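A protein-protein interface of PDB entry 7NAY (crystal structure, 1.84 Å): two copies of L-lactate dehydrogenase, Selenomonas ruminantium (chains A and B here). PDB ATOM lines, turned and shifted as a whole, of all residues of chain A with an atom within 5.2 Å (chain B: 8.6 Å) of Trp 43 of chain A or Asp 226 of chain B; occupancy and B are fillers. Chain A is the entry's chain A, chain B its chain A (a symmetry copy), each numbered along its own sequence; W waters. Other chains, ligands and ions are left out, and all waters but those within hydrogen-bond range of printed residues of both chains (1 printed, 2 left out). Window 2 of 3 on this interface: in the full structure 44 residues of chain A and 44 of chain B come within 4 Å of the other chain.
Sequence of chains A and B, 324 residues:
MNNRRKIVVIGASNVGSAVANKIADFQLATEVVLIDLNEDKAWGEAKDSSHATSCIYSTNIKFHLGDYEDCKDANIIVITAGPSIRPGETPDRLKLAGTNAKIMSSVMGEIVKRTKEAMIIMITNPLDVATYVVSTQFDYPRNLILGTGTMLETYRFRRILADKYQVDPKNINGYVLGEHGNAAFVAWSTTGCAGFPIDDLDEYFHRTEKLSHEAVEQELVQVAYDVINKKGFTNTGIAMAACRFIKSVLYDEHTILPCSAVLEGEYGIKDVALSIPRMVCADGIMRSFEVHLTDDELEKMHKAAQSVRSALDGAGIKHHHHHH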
ATOM      1  N   GLU A  39      -8.257  11.621  22.456  1.00  0.00           N
ATOM      2  CA  GLU A  39      -8.988  11.105  23.636  1.00  0.00           C
ATOM      3  C   GLU A  39      -8.496   9.686  23.947  1.00  0.00           C
ATOM      4  O   GLU A  39      -8.599   9.280  25.076  1.00  0.00           O
ATOM      5  CB  GLU A  39     -10.490  11.181  23.387  1.00  0.00           C
ATOM      6  CG  GLU A  39     -10.983  12.621  23.308  1.00  0.00           C
ATOM      7  CD  GLU A  39     -12.446  12.822  23.644  1.00  0.00           C
ATOM      8  OE1 GLU A  39     -13.257  11.913  23.336  1.00  0.00           O
ATOM      9  OE2 GLU A  39     -12.753  13.854  24.286  1.00  0.00           O
ATOM     10  N   ASP A  40      -8.025   8.945  22.950  1.00  0.00           N
ATOM     11  CA  ASP A  40      -7.494   7.578  23.159  1.00  0.00           C
ATOM     12  C   ASP A  40      -6.317   7.655  24.126  1.00  0.00           C
ATOM     13  O   ASP A  40      -6.270   6.871  25.066  1.00  0.00           O
ATOM     14  CB  ASP A  40      -7.070   6.916  21.861  1.00  0.00           C
ATOM     15  CG  ASP A  40      -8.229   6.312  21.082  1.00  0.00           C
ATOM     16  OD1 ASP A  40      -9.368   6.338  21.593  1.00  0.00           O
ATOM     17  OD2 ASP A  40      -7.971   5.860  19.955  1.00  0.00           O
ATOM     18  N   LYS A  41      -5.406   8.601  23.897  1.00  0.00           N
ATOM     19  CA  LYS A  41      -4.224   8.770  24.784  1.00  0.00           C
ATOM     20  C   LYS A  41      -4.702   9.157  26.186  1.00  0.00           C
ATOM     21  O   LYS A  41      -4.157   8.610  27.146  1.00  0.00           O
ATOM     22  CB  LYS A  41      -3.306   9.856  24.223  1.00  0.00           C
ATOM     23  CG  LYS A  41      -1.934   9.956  24.872  1.00  0.00           C
ATOM     24  CD  LYS A  41      -1.051   8.778  24.545  1.00  0.00           C
ATOM     25  CE  LYS A  41       0.337   8.900  25.130  1.00  0.00           C
ATOM     26  NZ  LYS A  41       0.350   9.794  26.311  1.00  0.00           N
ATOM     27  N   ALA A  42      -5.541  10.191  26.281  1.00  0.00           N
ATOM     28  CA  ALA A  42      -6.088  10.639  27.575  1.00  0.00           C
ATOM     29  C   ALA A  42      -6.722   9.442  28.315  1.00  0.00           C
ATOM     30  O   ALA A  42      -6.464   9.272  29.529  1.00  0.00           O
ATOM     31  CB  ALA A  42      -7.067  11.766  27.376  1.00  0.00           C
ATOM     32  N   TRP A  43      -7.494   8.614  27.611  1.00  0.00           N
ATOM     33  CA  TRP A  43      -8.177   7.440  28.199  1.00  0.00           C
ATOM     34  C   TRP A  43      -7.114   6.441  28.677  1.00  0.00           C
ATOM     35  O   TRP A  43      -7.244   5.903  29.815  1.00  0.00           O
ATOM     36  CB  TRP A  43      -9.148   6.815  27.188  1.00  0.00           C
ATOM     37  CG  TRP A  43      -9.799   5.577  27.708  1.00  0.00           C
ATOM     38  CD1 TRP A  43     -11.017   5.498  28.321  1.00  0.00           C
ATOM     39  CD2 TRP A  43      -9.278   4.237  27.671  1.00  0.00           C
ATOM     40  NE1 TRP A  43     -11.265   4.215  28.710  1.00  0.00           N
ATOM     41  CE2 TRP A  43     -10.249   3.414  28.287  1.00  0.00           C
ATOM     42  CE3 TRP A  43      -8.122   3.641  27.149  1.00  0.00           C
ATOM     43  CZ2 TRP A  43     -10.068   2.043  28.448  1.00  0.00           C
ATOM     44  CZ3 TRP A  43      -7.948   2.279  27.296  1.00  0.00           C
ATOM     45  CH2 TRP A  43      -8.917   1.496  27.928  1.00  0.00           C
ATOM     46  N   GLY A  44      -6.136   6.126  27.831  1.00  0.00           N
ATOM     47  CA  GLY A  44      -5.081   5.162  28.193  1.00  0.00           C
ATOM     48  C   GLY A  44      -4.287   5.608  29.425  1.00  0.00           C
ATOM     49  O   GLY A  44      -4.025   4.766  30.296  1.00  0.00           O
ATOM     50  N   GLU A  45      -3.847   6.865  29.437  1.00  0.00           N
ATOM     51  CA  GLU A  45      -3.128   7.491  30.588  1.00  0.00           C
ATOM     52  C   GLU A  45      -3.961   7.392  31.862  1.00  0.00           C
ATOM     53  O   GLU A  45      -3.463   6.887  32.870  1.00  0.00           O
ATOM     54  CB  GLU A  45      -2.808   8.943  30.248  1.00  0.00           C
ATOM     55  CG  GLU A  45      -1.652   9.083  29.306  1.00  0.00           C
ATOM     56  CD  GLU A  45      -0.313   8.556  29.786  1.00  0.00           C
ATOM     57  OE1 GLU A  45      -0.215   8.104  30.962  1.00  0.00           O
ATOM     58  OE2 GLU A  45       0.637   8.635  28.990  1.00  0.00           O
ATOM     59  N   ALA A  46      -5.238   7.770  31.781  1.00  0.00           N
ATOM     60  CA  ALA A  46      -6.162   7.717  32.923  1.00  0.00           C
ATOM     61  C   ALA A  46      -6.360   6.262  33.374  1.00  0.00           C
ATOM     62  O   ALA A  46      -6.315   5.985  34.599  1.00  0.00           O
ATOM     63  CB  ALA A  46      -7.466   8.406  32.581  1.00  0.00           C
ATOM     64  N   LYS A  47      -6.446   5.320  32.442  1.00  0.00           N
ATOM     65  CA  LYS A  47      -6.656   3.911  32.822  1.00  0.00           C
ATOM     66  C   LYS A  47      -5.414   3.374  33.556  1.00  0.00           C
ATOM     67  O   LYS A  47      -5.550   2.725  34.634  1.00  0.00           O
ATOM     68  CB  LYS A  47      -7.036   3.121  31.566  1.00  0.00           C
ATOM     69  CG  LYS A  47      -7.421   1.692  31.809  1.00  0.00           C
ATOM     70  CD  LYS A  47      -8.701   1.487  32.622  1.00  0.00           C
ATOM     71  CE  LYS A  47      -9.951   2.116  32.076  1.00  0.00           C
ATOM     72  NZ  LYS A  47     -11.137   1.603  32.838  1.00  0.00           N
ATOM     73  N   ASP A  48      -4.235   3.616  32.990  1.00  0.00           N
ATOM     74  CA  ASP A  48      -2.951   3.176  33.588  1.00  0.00           C
ATOM     75  C   ASP A  48      -2.860   3.770  35.010  1.00  0.00           C
ATOM     76  O   ASP A  48      -2.611   3.006  35.965  1.00  0.00           O
ATOM     77  CB  ASP A  48      -1.818   3.633  32.697  1.00  0.00           C
ATOM     78  CG  ASP A  48      -0.529   2.869  32.867  1.00  0.00           C
ATOM     79  OD1 ASP A  48      -0.501   1.907  33.697  1.00  0.00           O
ATOM     80  OD2 ASP A  48       0.412   3.232  32.145  1.00  0.00           O
ATOM     81  N   LEU A  65     -10.696   9.960  31.515  1.00  0.00           N
ATOM     82  CA  LEU A  65     -10.860  10.847  30.347  1.00  0.00           C
ATOM     83  C   LEU A  65     -11.999  11.799  30.673  1.00  0.00           C
ATOM     84  O   LEU A  65     -12.989  11.372  31.249  1.00  0.00           O
ATOM     85  CB  LEU A  65     -11.194  10.000  29.126  1.00  0.00           C
ATOM     86  CG  LEU A  65     -11.743  10.761  27.933  1.00  0.00           C
ATOM     87  CD1 LEU A  65     -10.657  11.677  27.383  1.00  0.00           C
ATOM     88  CD2 LEU A  65     -12.198   9.758  26.884  1.00  0.00           C
ATOM     89  N   ILE B  85       5.490  -5.392  23.544  1.00  0.00           N
ATOM     90  CA  ILE B  85       4.539  -5.544  22.418  1.00  0.00           C
ATOM     91  C   ILE B  85       4.040  -4.138  22.076  1.00  0.00           C
ATOM     92  O   ILE B  85       3.924  -3.252  22.962  1.00  0.00           O
ATOM     93  CB  ILE B  85       3.427  -6.553  22.734  1.00  0.00           C
ATOM     94  CG1 ILE B  85       2.582  -6.138  23.931  1.00  0.00           C
ATOM     95  CG2 ILE B  85       4.005  -7.966  22.882  1.00  0.00           C
ATOM     96  CD1 ILE B  85       1.533  -7.162  24.311  1.00  0.00           C
ATOM     97  N   PRO B  87       1.578  -1.269  19.687  1.00  0.00           N
ATOM     98  CA  PRO B  87       0.217  -1.138  19.186  1.00  0.00           C
ATOM     99  C   PRO B  87      -0.002  -1.920  17.875  1.00  0.00           C
ATOM    100  O   PRO B  87       0.875  -1.937  17.025  1.00  0.00           O
ATOM    101  CB  PRO B  87       0.055   0.365  18.976  1.00  0.00           C
ATOM    102  CG  PRO B  87       1.014   0.995  19.966  1.00  0.00           C
ATOM    103  CD  PRO B  87       2.166   0.008  20.131  1.00  0.00           C
ATOM    104  N   PRO B  91      -1.600  -9.505  20.556  1.00  0.00           N
ATOM    105  CA  PRO B  91      -1.693  -9.272  22.002  1.00  0.00           C
ATOM    106  C   PRO B  91      -1.201 -10.495  22.774  1.00  0.00           C
ATOM    107  O   PRO B  91      -1.980 -11.213  23.338  1.00  0.00           O
ATOM    108  CB  PRO B  91      -3.200  -9.025  22.233  1.00  0.00           C
ATOM    109  CG  PRO B  91      -3.892  -9.741  21.072  1.00  0.00           C
ATOM    110  CD  PRO B  91      -2.927  -9.578  19.911  1.00  0.00           C
ATOM    111  N   ARG B  93       2.339 -11.284  25.078  1.00  0.00           N
ATOM    112  CA  ARG B  93       3.668 -10.947  25.629  1.00  0.00           C
ATOM    113  C   ARG B  93       4.632 -12.114  25.382  1.00  0.00           C
ATOM    114  O   ARG B  93       5.822 -11.857  25.271  1.00  0.00           O
ATOM    115  CB  ARG B  93       3.524 -10.650  27.120  1.00  0.00           C
ATOM    116  CG  ARG B  93       2.693  -9.416  27.446  1.00  0.00           C
ATOM    117  CD  ARG B  93       2.438  -9.485  28.925  1.00  0.00           C
ATOM    118  NE  ARG B  93       1.645  -8.375  29.449  1.00  0.00           N
ATOM    119  CZ  ARG B  93       0.335  -8.347  29.436  1.00  0.00           C
ATOM    120  NH1 ARG B  93      -0.333  -9.306  28.822  1.00  0.00           N
ATOM    121  NH2 ARG B  93      -0.324  -7.363  30.032  1.00  0.00           N
ATOM    122  N   GLN B 218     -11.806 -11.268  31.796  1.00  0.00           N
ATOM    123  CA  GLN B 218     -11.375 -10.870  30.425  1.00  0.00           C
ATOM    124  C   GLN B 218     -11.024  -9.378  30.405  1.00  0.00           C
ATOM    125  O   GLN B 218     -10.108  -9.003  29.695  1.00  0.00           O
ATOM    126  CB  GLN B 218     -12.462 -11.222  29.423  1.00  0.00           C
ATOM    127  CG  GLN B 218     -12.459 -12.721  29.249  1.00  0.00           C
ATOM    128  CD  GLN B 218     -13.659 -13.217  28.502  1.00  0.00           C
ATOM    129  OE1 GLN B 218     -14.302 -12.455  27.766  1.00  0.00           O
ATOM    130  NE2 GLN B 218     -13.940 -14.497  28.708  1.00  0.00           N
ATOM    131  N   GLU B 219     -11.790  -8.560  31.108  1.00  0.00           N
ATOM    132  CA  GLU B 219     -11.542  -7.092  31.117  1.00  0.00           C
ATOM    133  C   GLU B 219     -10.148  -6.811  31.681  1.00  0.00           C
ATOM    134  O   GLU B 219      -9.394  -6.014  31.073  1.00  0.00           O
ATOM    135  CB  GLU B 219     -12.609  -6.347  31.904  1.00  0.00           C
ATOM    136  CG  GLU B 219     -12.420  -4.844  31.756  1.00  0.00           C
ATOM    137  CD  GLU B 219     -13.506  -4.013  32.404  1.00  0.00           C
ATOM    138  OE1 GLU B 219     -14.623  -4.541  32.596  1.00  0.00           O
ATOM    139  OE2 GLU B 219     -13.238  -2.865  32.740  1.00  0.00           O
ATOM    140  N   LEU B 220      -9.783  -7.468  32.777  1.00  0.00           N
ATOM    141  CA  LEU B 220      -8.532  -7.133  33.496  1.00  0.00           C
ATOM    142  C   LEU B 220      -7.370  -7.583  32.622  1.00  0.00           C
ATOM    143  O   LEU B 220      -6.270  -6.984  32.702  1.00  0.00           O
ATOM    144  CB  LEU B 220      -8.524  -7.777  34.895  1.00  0.00           C
ATOM    145  CG  LEU B 220      -8.285  -9.270  35.017  1.00  0.00           C
ATOM    146  CD1 LEU B 220      -6.798  -9.610  35.082  1.00  0.00           C
ATOM    147  CD2 LEU B 220      -8.984  -9.777  36.274  1.00  0.00           C
ATOM    148  N   VAL B 221      -7.601  -8.582  31.777  1.00  0.00           N
ATOM    149  CA  VAL B 221      -6.544  -9.003  30.825  1.00  0.00           C
ATOM    150  C   VAL B 221      -6.510  -8.046  29.642  1.00  0.00           C
ATOM    151  O   VAL B 221      -5.409  -7.588  29.295  1.00  0.00           O
ATOM    152  CB  VAL B 221      -6.695 -10.457  30.347  1.00  0.00           C
ATOM    153  CG1 VAL B 221      -5.694 -10.729  29.248  1.00  0.00           C
ATOM    154  CG2 VAL B 221      -6.511 -11.442  31.479  1.00  0.00           C
ATOM    155  N   GLN B 222      -7.666  -7.789  29.037  1.00  0.00           N
ATOM    156  CA  GLN B 222      -7.780  -7.038  27.769  1.00  0.00           C
ATOM    157  C   GLN B 222      -7.364  -5.579  28.010  1.00  0.00           C
ATOM    158  O   GLN B 222      -6.834  -4.915  27.089  1.00  0.00           O
ATOM    159  CB  GLN B 222      -9.217  -7.120  27.253  1.00  0.00           C
ATOM    160  CG  GLN B 222      -9.429  -6.294  25.988  1.00  0.00           C
ATOM    161  CD  GLN B 222      -8.551  -6.752  24.859  1.00  0.00           C
ATOM    162  OE1 GLN B 222      -8.308  -7.951  24.676  1.00  0.00           O
ATOM    163  NE2 GLN B 222      -8.123  -5.796  24.038  1.00  0.00           N
ATOM    164  N   VAL B 223      -7.591  -5.046  29.204  1.00  0.00           N
ATOM    165  CA  VAL B 223      -7.344  -3.588  29.403  1.00  0.00           C
ATOM    166  C   VAL B 223      -5.862  -3.285  29.153  1.00  0.00           C
ATOM    167  O   VAL B 223      -5.592  -2.157  28.729  1.00  0.00           O
ATOM    168  CB  VAL B 223      -7.825  -3.082  30.769  1.00  0.00           C
ATOM    169  CG1 VAL B 223      -7.046  -3.657  31.931  1.00  0.00           C
ATOM    170  CG2 VAL B 223      -7.840  -1.561  30.814  1.00  0.00           C
ATOM    171  N   ALA B 224      -4.935  -4.203  29.436  1.00  0.00           N
ATOM    172  CA  ALA B 224      -3.485  -3.968  29.197  1.00  0.00           C
ATOM    173  C   ALA B 224      -3.259  -3.679  27.703  1.00  0.00           C
ATOM    174  O   ALA B 224      -2.553  -2.709  27.345  1.00  0.00           O
ATOM    175  CB  ALA B 224      -2.681  -5.122  29.702  1.00  0.00           C
ATOM    176  N   TYR B 225      -3.911  -4.460  26.846  1.00  0.00           N
ATOM    177  CA  TYR B 225      -3.762  -4.274  25.381  1.00  0.00           C
ATOM    178  C   TYR B 225      -4.454  -2.982  24.928  1.00  0.00           C
ATOM    179  O   TYR B 225      -3.905  -2.285  24.073  1.00  0.00           O
ATOM    180  CB  TYR B 225      -4.283  -5.504  24.639  1.00  0.00           C
ATOM    181  CG  TYR B 225      -3.736  -6.809  25.152  1.00  0.00           C
ATOM    182  CD1 TYR B 225      -2.372  -7.028  25.220  1.00  0.00           C
ATOM    183  CD2 TYR B 225      -4.578  -7.821  25.576  1.00  0.00           C
ATOM    184  CE1 TYR B 225      -1.854  -8.218  25.697  1.00  0.00           C
ATOM    185  CE2 TYR B 225      -4.078  -9.019  26.053  1.00  0.00           C
ATOM    186  CZ  TYR B 225      -2.711  -9.218  26.110  1.00  0.00           C
ATOM    187  OH  TYR B 225      -2.206 -10.393  26.574  1.00  0.00           O
ATOM    188  N   ASP B 226      -5.615  -2.680  25.508  1.00  0.00           N
ATOM    189  CA  ASP B 226      -6.274  -1.404  25.132  1.00  0.00           C
ATOM    190  C   ASP B 226      -5.360  -0.216  25.498  1.00  0.00           C
ATOM    191  O   ASP B 226      -5.182   0.719  24.666  1.00  0.00           O
ATOM    192  CB  ASP B 226      -7.649  -1.278  25.762  1.00  0.00           C
ATOM    193  CG  ASP B 226      -8.628  -2.325  25.273  1.00  0.00           C
ATOM    194  OD1 ASP B 226      -8.376  -2.905  24.205  1.00  0.00           O
ATOM    195  OD2 ASP B 226      -9.608  -2.568  25.987  1.00  0.00           O
ATOM    196  N   VAL B 227      -4.750  -0.238  26.670  1.00  0.00           N
ATOM    197  CA  VAL B 227      -3.843   0.879  27.089  1.00  0.00           C
ATOM    198  C   VAL B 227      -2.643   0.934  26.129  1.00  0.00           C
ATOM    199  O   VAL B 227      -2.239   2.047  25.738  1.00  0.00           O
ATOM    200  CB  VAL B 227      -3.418   0.760  28.558  1.00  0.00           C
ATOM    201  CG1 VAL B 227      -2.373   1.808  28.920  1.00  0.00           C
ATOM    202  CG2 VAL B 227      -4.630   0.885  29.451  1.00  0.00           C
ATOM    203  N   ILE B 228      -2.073  -0.219  25.780  1.00  0.00           N
ATOM    204  CA  ILE B 228      -0.904  -0.229  24.865  1.00  0.00           C
ATOM    205  C   ILE B 228      -1.333   0.389  23.539  1.00  0.00           C
ATOM    206  O   ILE B 228      -0.578   1.209  23.032  1.00  0.00           O
ATOM    207  CB  ILE B 228      -0.293  -1.620  24.698  1.00  0.00           C
ATOM    208  CG1 ILE B 228       0.380  -2.072  26.003  1.00  0.00           C
ATOM    209  CG2 ILE B 228       0.701  -1.622  23.537  1.00  0.00           C
ATOM    210  CD1 ILE B 228       0.743  -3.525  25.995  1.00  0.00           C
ATOM    211  N   ASN B 229      -2.485  -0.019  23.006  1.00  0.00           N
ATOM    212  CA  ASN B 229      -3.002   0.482  21.706  1.00  0.00           C
ATOM    213  C   ASN B 229      -3.294   1.981  21.771  1.00  0.00           C
ATOM    214  O   ASN B 229      -3.068   2.644  20.744  1.00  0.00           O
ATOM    215  CB  ASN B 229      -4.225  -0.301  21.217  1.00  0.00           C
ATOM    216  CG  ASN B 229      -3.881  -1.733  20.852  1.00  0.00           C
ATOM    217  OD1 ASN B 229      -2.770  -2.033  20.427  1.00  0.00           O
ATOM    218  ND2 ASN B 229      -4.822  -2.645  21.033  1.00  0.00           N
ATOM    219  N   LYS B 230      -3.749   2.513  22.913  1.00  0.00           N
ATOM    220  CA  LYS B 230      -4.315   3.890  22.984  1.00  0.00           C
ATOM    221  C   LYS B 230      -3.285   4.870  23.547  1.00  0.00           C
ATOM    222  O   LYS B 230      -3.247   6.020  23.044  1.00  0.00           O
ATOM    223  CB  LYS B 230      -5.642   3.862  23.723  1.00  0.00           C
ATOM    224  CG  LYS B 230      -6.710   3.164  22.890  1.00  0.00           C
ATOM    225  CD  LYS B 230      -8.089   3.183  23.488  1.00  0.00           C
ATOM    226  CE  LYS B 230      -9.153   2.824  22.456  1.00  0.00           C
ATOM    227  NZ  LYS B 230     -10.499   3.215  22.943  1.00  0.00           N
ATOM    228  N   LYS B 231      -2.435   4.400  24.457  1.00  0.00           N
ATOM    229  CA  LYS B 231      -1.393   5.234  25.088  1.00  0.00           C
ATOM    230  C   LYS B 231      -0.074   4.953  24.364  1.00  0.00           C
ATOM    231  O   LYS B 231       0.752   5.876  24.320  1.00  0.00           O
ATOM    232  CB  LYS B 231      -1.362   4.972  26.596  1.00  0.00           C
ATOM    233  CG  LYS B 231      -0.144   5.526  27.316  1.00  0.00           C
ATOM    234  CD  LYS B 231      -0.120   5.180  28.810  1.00  0.00           C
ATOM    235  CE  LYS B 231       1.250   5.379  29.438  1.00  0.00           C
ATOM    236  NZ  LYS B 231       1.177   5.761  30.855  1.00  0.00           N
ATOM    237  N   GLY B 232       0.116   3.733  23.822  1.00  0.00           N
ATOM    238  CA  GLY B 232       1.334   3.313  23.102  1.00  0.00           C
ATOM    239  C   GLY B 232       2.151   2.287  23.871  1.00  0.00           C
ATOM    240  O   GLY B 232       3.055   1.646  23.269  1.00  0.00           O
ATOM    241  N   PHE B 233       1.898   2.211  25.181  1.00  0.00           N
ATOM    242  CA  PHE B 233       2.695   1.448  26.179  1.00  0.00           C
ATOM    243  C   PHE B 233       1.970   1.589  27.530  1.00  0.00           C
ATOM    244  O   PHE B 233       0.966   2.324  27.595  1.00  0.00           O
ATOM    245  CB  PHE B 233       4.127   1.984  26.228  1.00  0.00           C
ATOM    246  CG  PHE B 233       4.205   3.449  26.568  1.00  0.00           C
ATOM    247  CD1 PHE B 233       4.175   4.408  25.567  1.00  0.00           C
ATOM    248  CD2 PHE B 233       4.279   3.869  27.891  1.00  0.00           C
ATOM    249  CE1 PHE B 233       4.245   5.761  25.877  1.00  0.00           C
ATOM    250  CE2 PHE B 233       4.357   5.223  28.203  1.00  0.00           C
ATOM    251  CZ  PHE B 233       4.304   6.169  27.202  1.00  0.00           C
ATOM    252  N   THR B 234       2.464   0.893  28.551  1.00  0.00           N
ATOM    253  CA  THR B 234       1.954   1.100  29.931  1.00  0.00           C
ATOM    254  C   THR B 234       3.181   1.364  30.818  1.00  0.00           C
ATOM    255  O   THR B 234       4.259   0.891  30.475  1.00  0.00           O
ATOM    256  CB  THR B 234       1.233  -0.115  30.526  1.00  0.00           C
ATOM    257  OG1 THR B 234       2.184  -1.026  31.070  1.00  0.00           O
ATOM    258  CG2 THR B 234       0.306  -0.791  29.540  1.00  0.00           C
HETATM  259  O   HOH W   1       1.542  -0.056  33.851  1.00  0.00           O
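No position is printed for both chains.
Of the 11 pairs that touch across the chains among the printed residues, none has its exchanged pair printed and touching as well.
The side-chain amino group of Lys 41 of chain A lies within salt-bridge range of the side-chain carboxylate of Glu 45 of chain A (2.9 Å).
The side-chain amide nitrogen (NE2) of Gln 222 of chain B is in hydrogen-bond range of the side-chain carboxylate (OD1) of Asp 226 of chain B, at 2.9 Å.
The backbone carbonyl oxygen of Val 227 of chain B is in hydrogen-bond range of the backbone NH of Gly 232 of chain B, 3.5 Å away.
Water W1 bridges OD1 of Asp 48 of chain A (2.8 Å) and OG1 of Thr 234 of chain B (3.0 Å).
Of the printed residues of chain B, Glu 45 of chain A touches Lys 231.
Of the printed residues of chain B, Lys 47 of chain A touches Val 223 (3.4 Å) and Val 227 (3.7 Å).
Of the printed residues of chain B, Asp 40 of chain A touches Lys 230 (3.4 Å).
Printed residues of chain A within 4 Å of Val 223 of chain B: Lys 47.
Ala 46 of chain A touches none of the printed residues of chain B.
The nearest residue of chain B that does not touch Trp 43 of chain A is Val 227 of chain B (4.1 Å).
Among the printed residues, merely in contact across the chains: Lys 41 of chain A with Lys 231 of chain B (3.2 Å), Lys 47 of chain A with Val 223 of chain B (3.4 Å), Asp 48 of chain A with Thr 234 of chain B (3.4 Å), Gly 44 of chain A with Val 227 of chain B (3.7 Å), Trp 43 of chain A with Lys 230 of chain B (3.7 Å), Trp 43 of chain A with Asp 226 of chain B (3.7 Å) and Lys 47 of chain A with Val 227 of chain B (3.7 Å).
The side-chain carboxylate (OD1) of Asp 40 of chain A lies within salt-bridge range of the side-chain amino group (NZ) of Lys 230 of chain B (3.6 Å).
The backbone NH (N) of Lys 41 of chain A lies close to the backbone carbonyl oxygen (O) of Lys 230 of chain B, at 3.5 Å.
OE1 of Glu 45 of chain A is in salt-bridge range of NZ of Lys 231 of chain B (2.7 Å).
The side-chain amino group (NZ) of Lys 231 of chain B is in salt-bridge range of the side-chain carboxylate (OD2) of Asp 48 of chain A (2.9 Å).
Hydrophobic or aromatic side chains of chain B within 4 Å of the printed part of chain A: Val 223 and Val 227.
Of the 11 printed residues of chain A, 7 touch a printed residue of chain B.
Printed residues of chain A that touch a printed residue of chain B: Asp 40, Lys 41, Trp 43, Gly 44, Glu 45, Lys 47 and Asp 48.
Among the printed residues, 11 pairs touch across the chains.
Among the printed residues, Asp or Glu carboxylates within 4 Å of a Lys or Arg side-chain nitrogen of the other chain: Asp 40 of chain A with Lys 230 of chain B, Glu 45 of chain A with Lys 231 of chain B and Asp 48 of chain A with Lys 231 of chain B.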
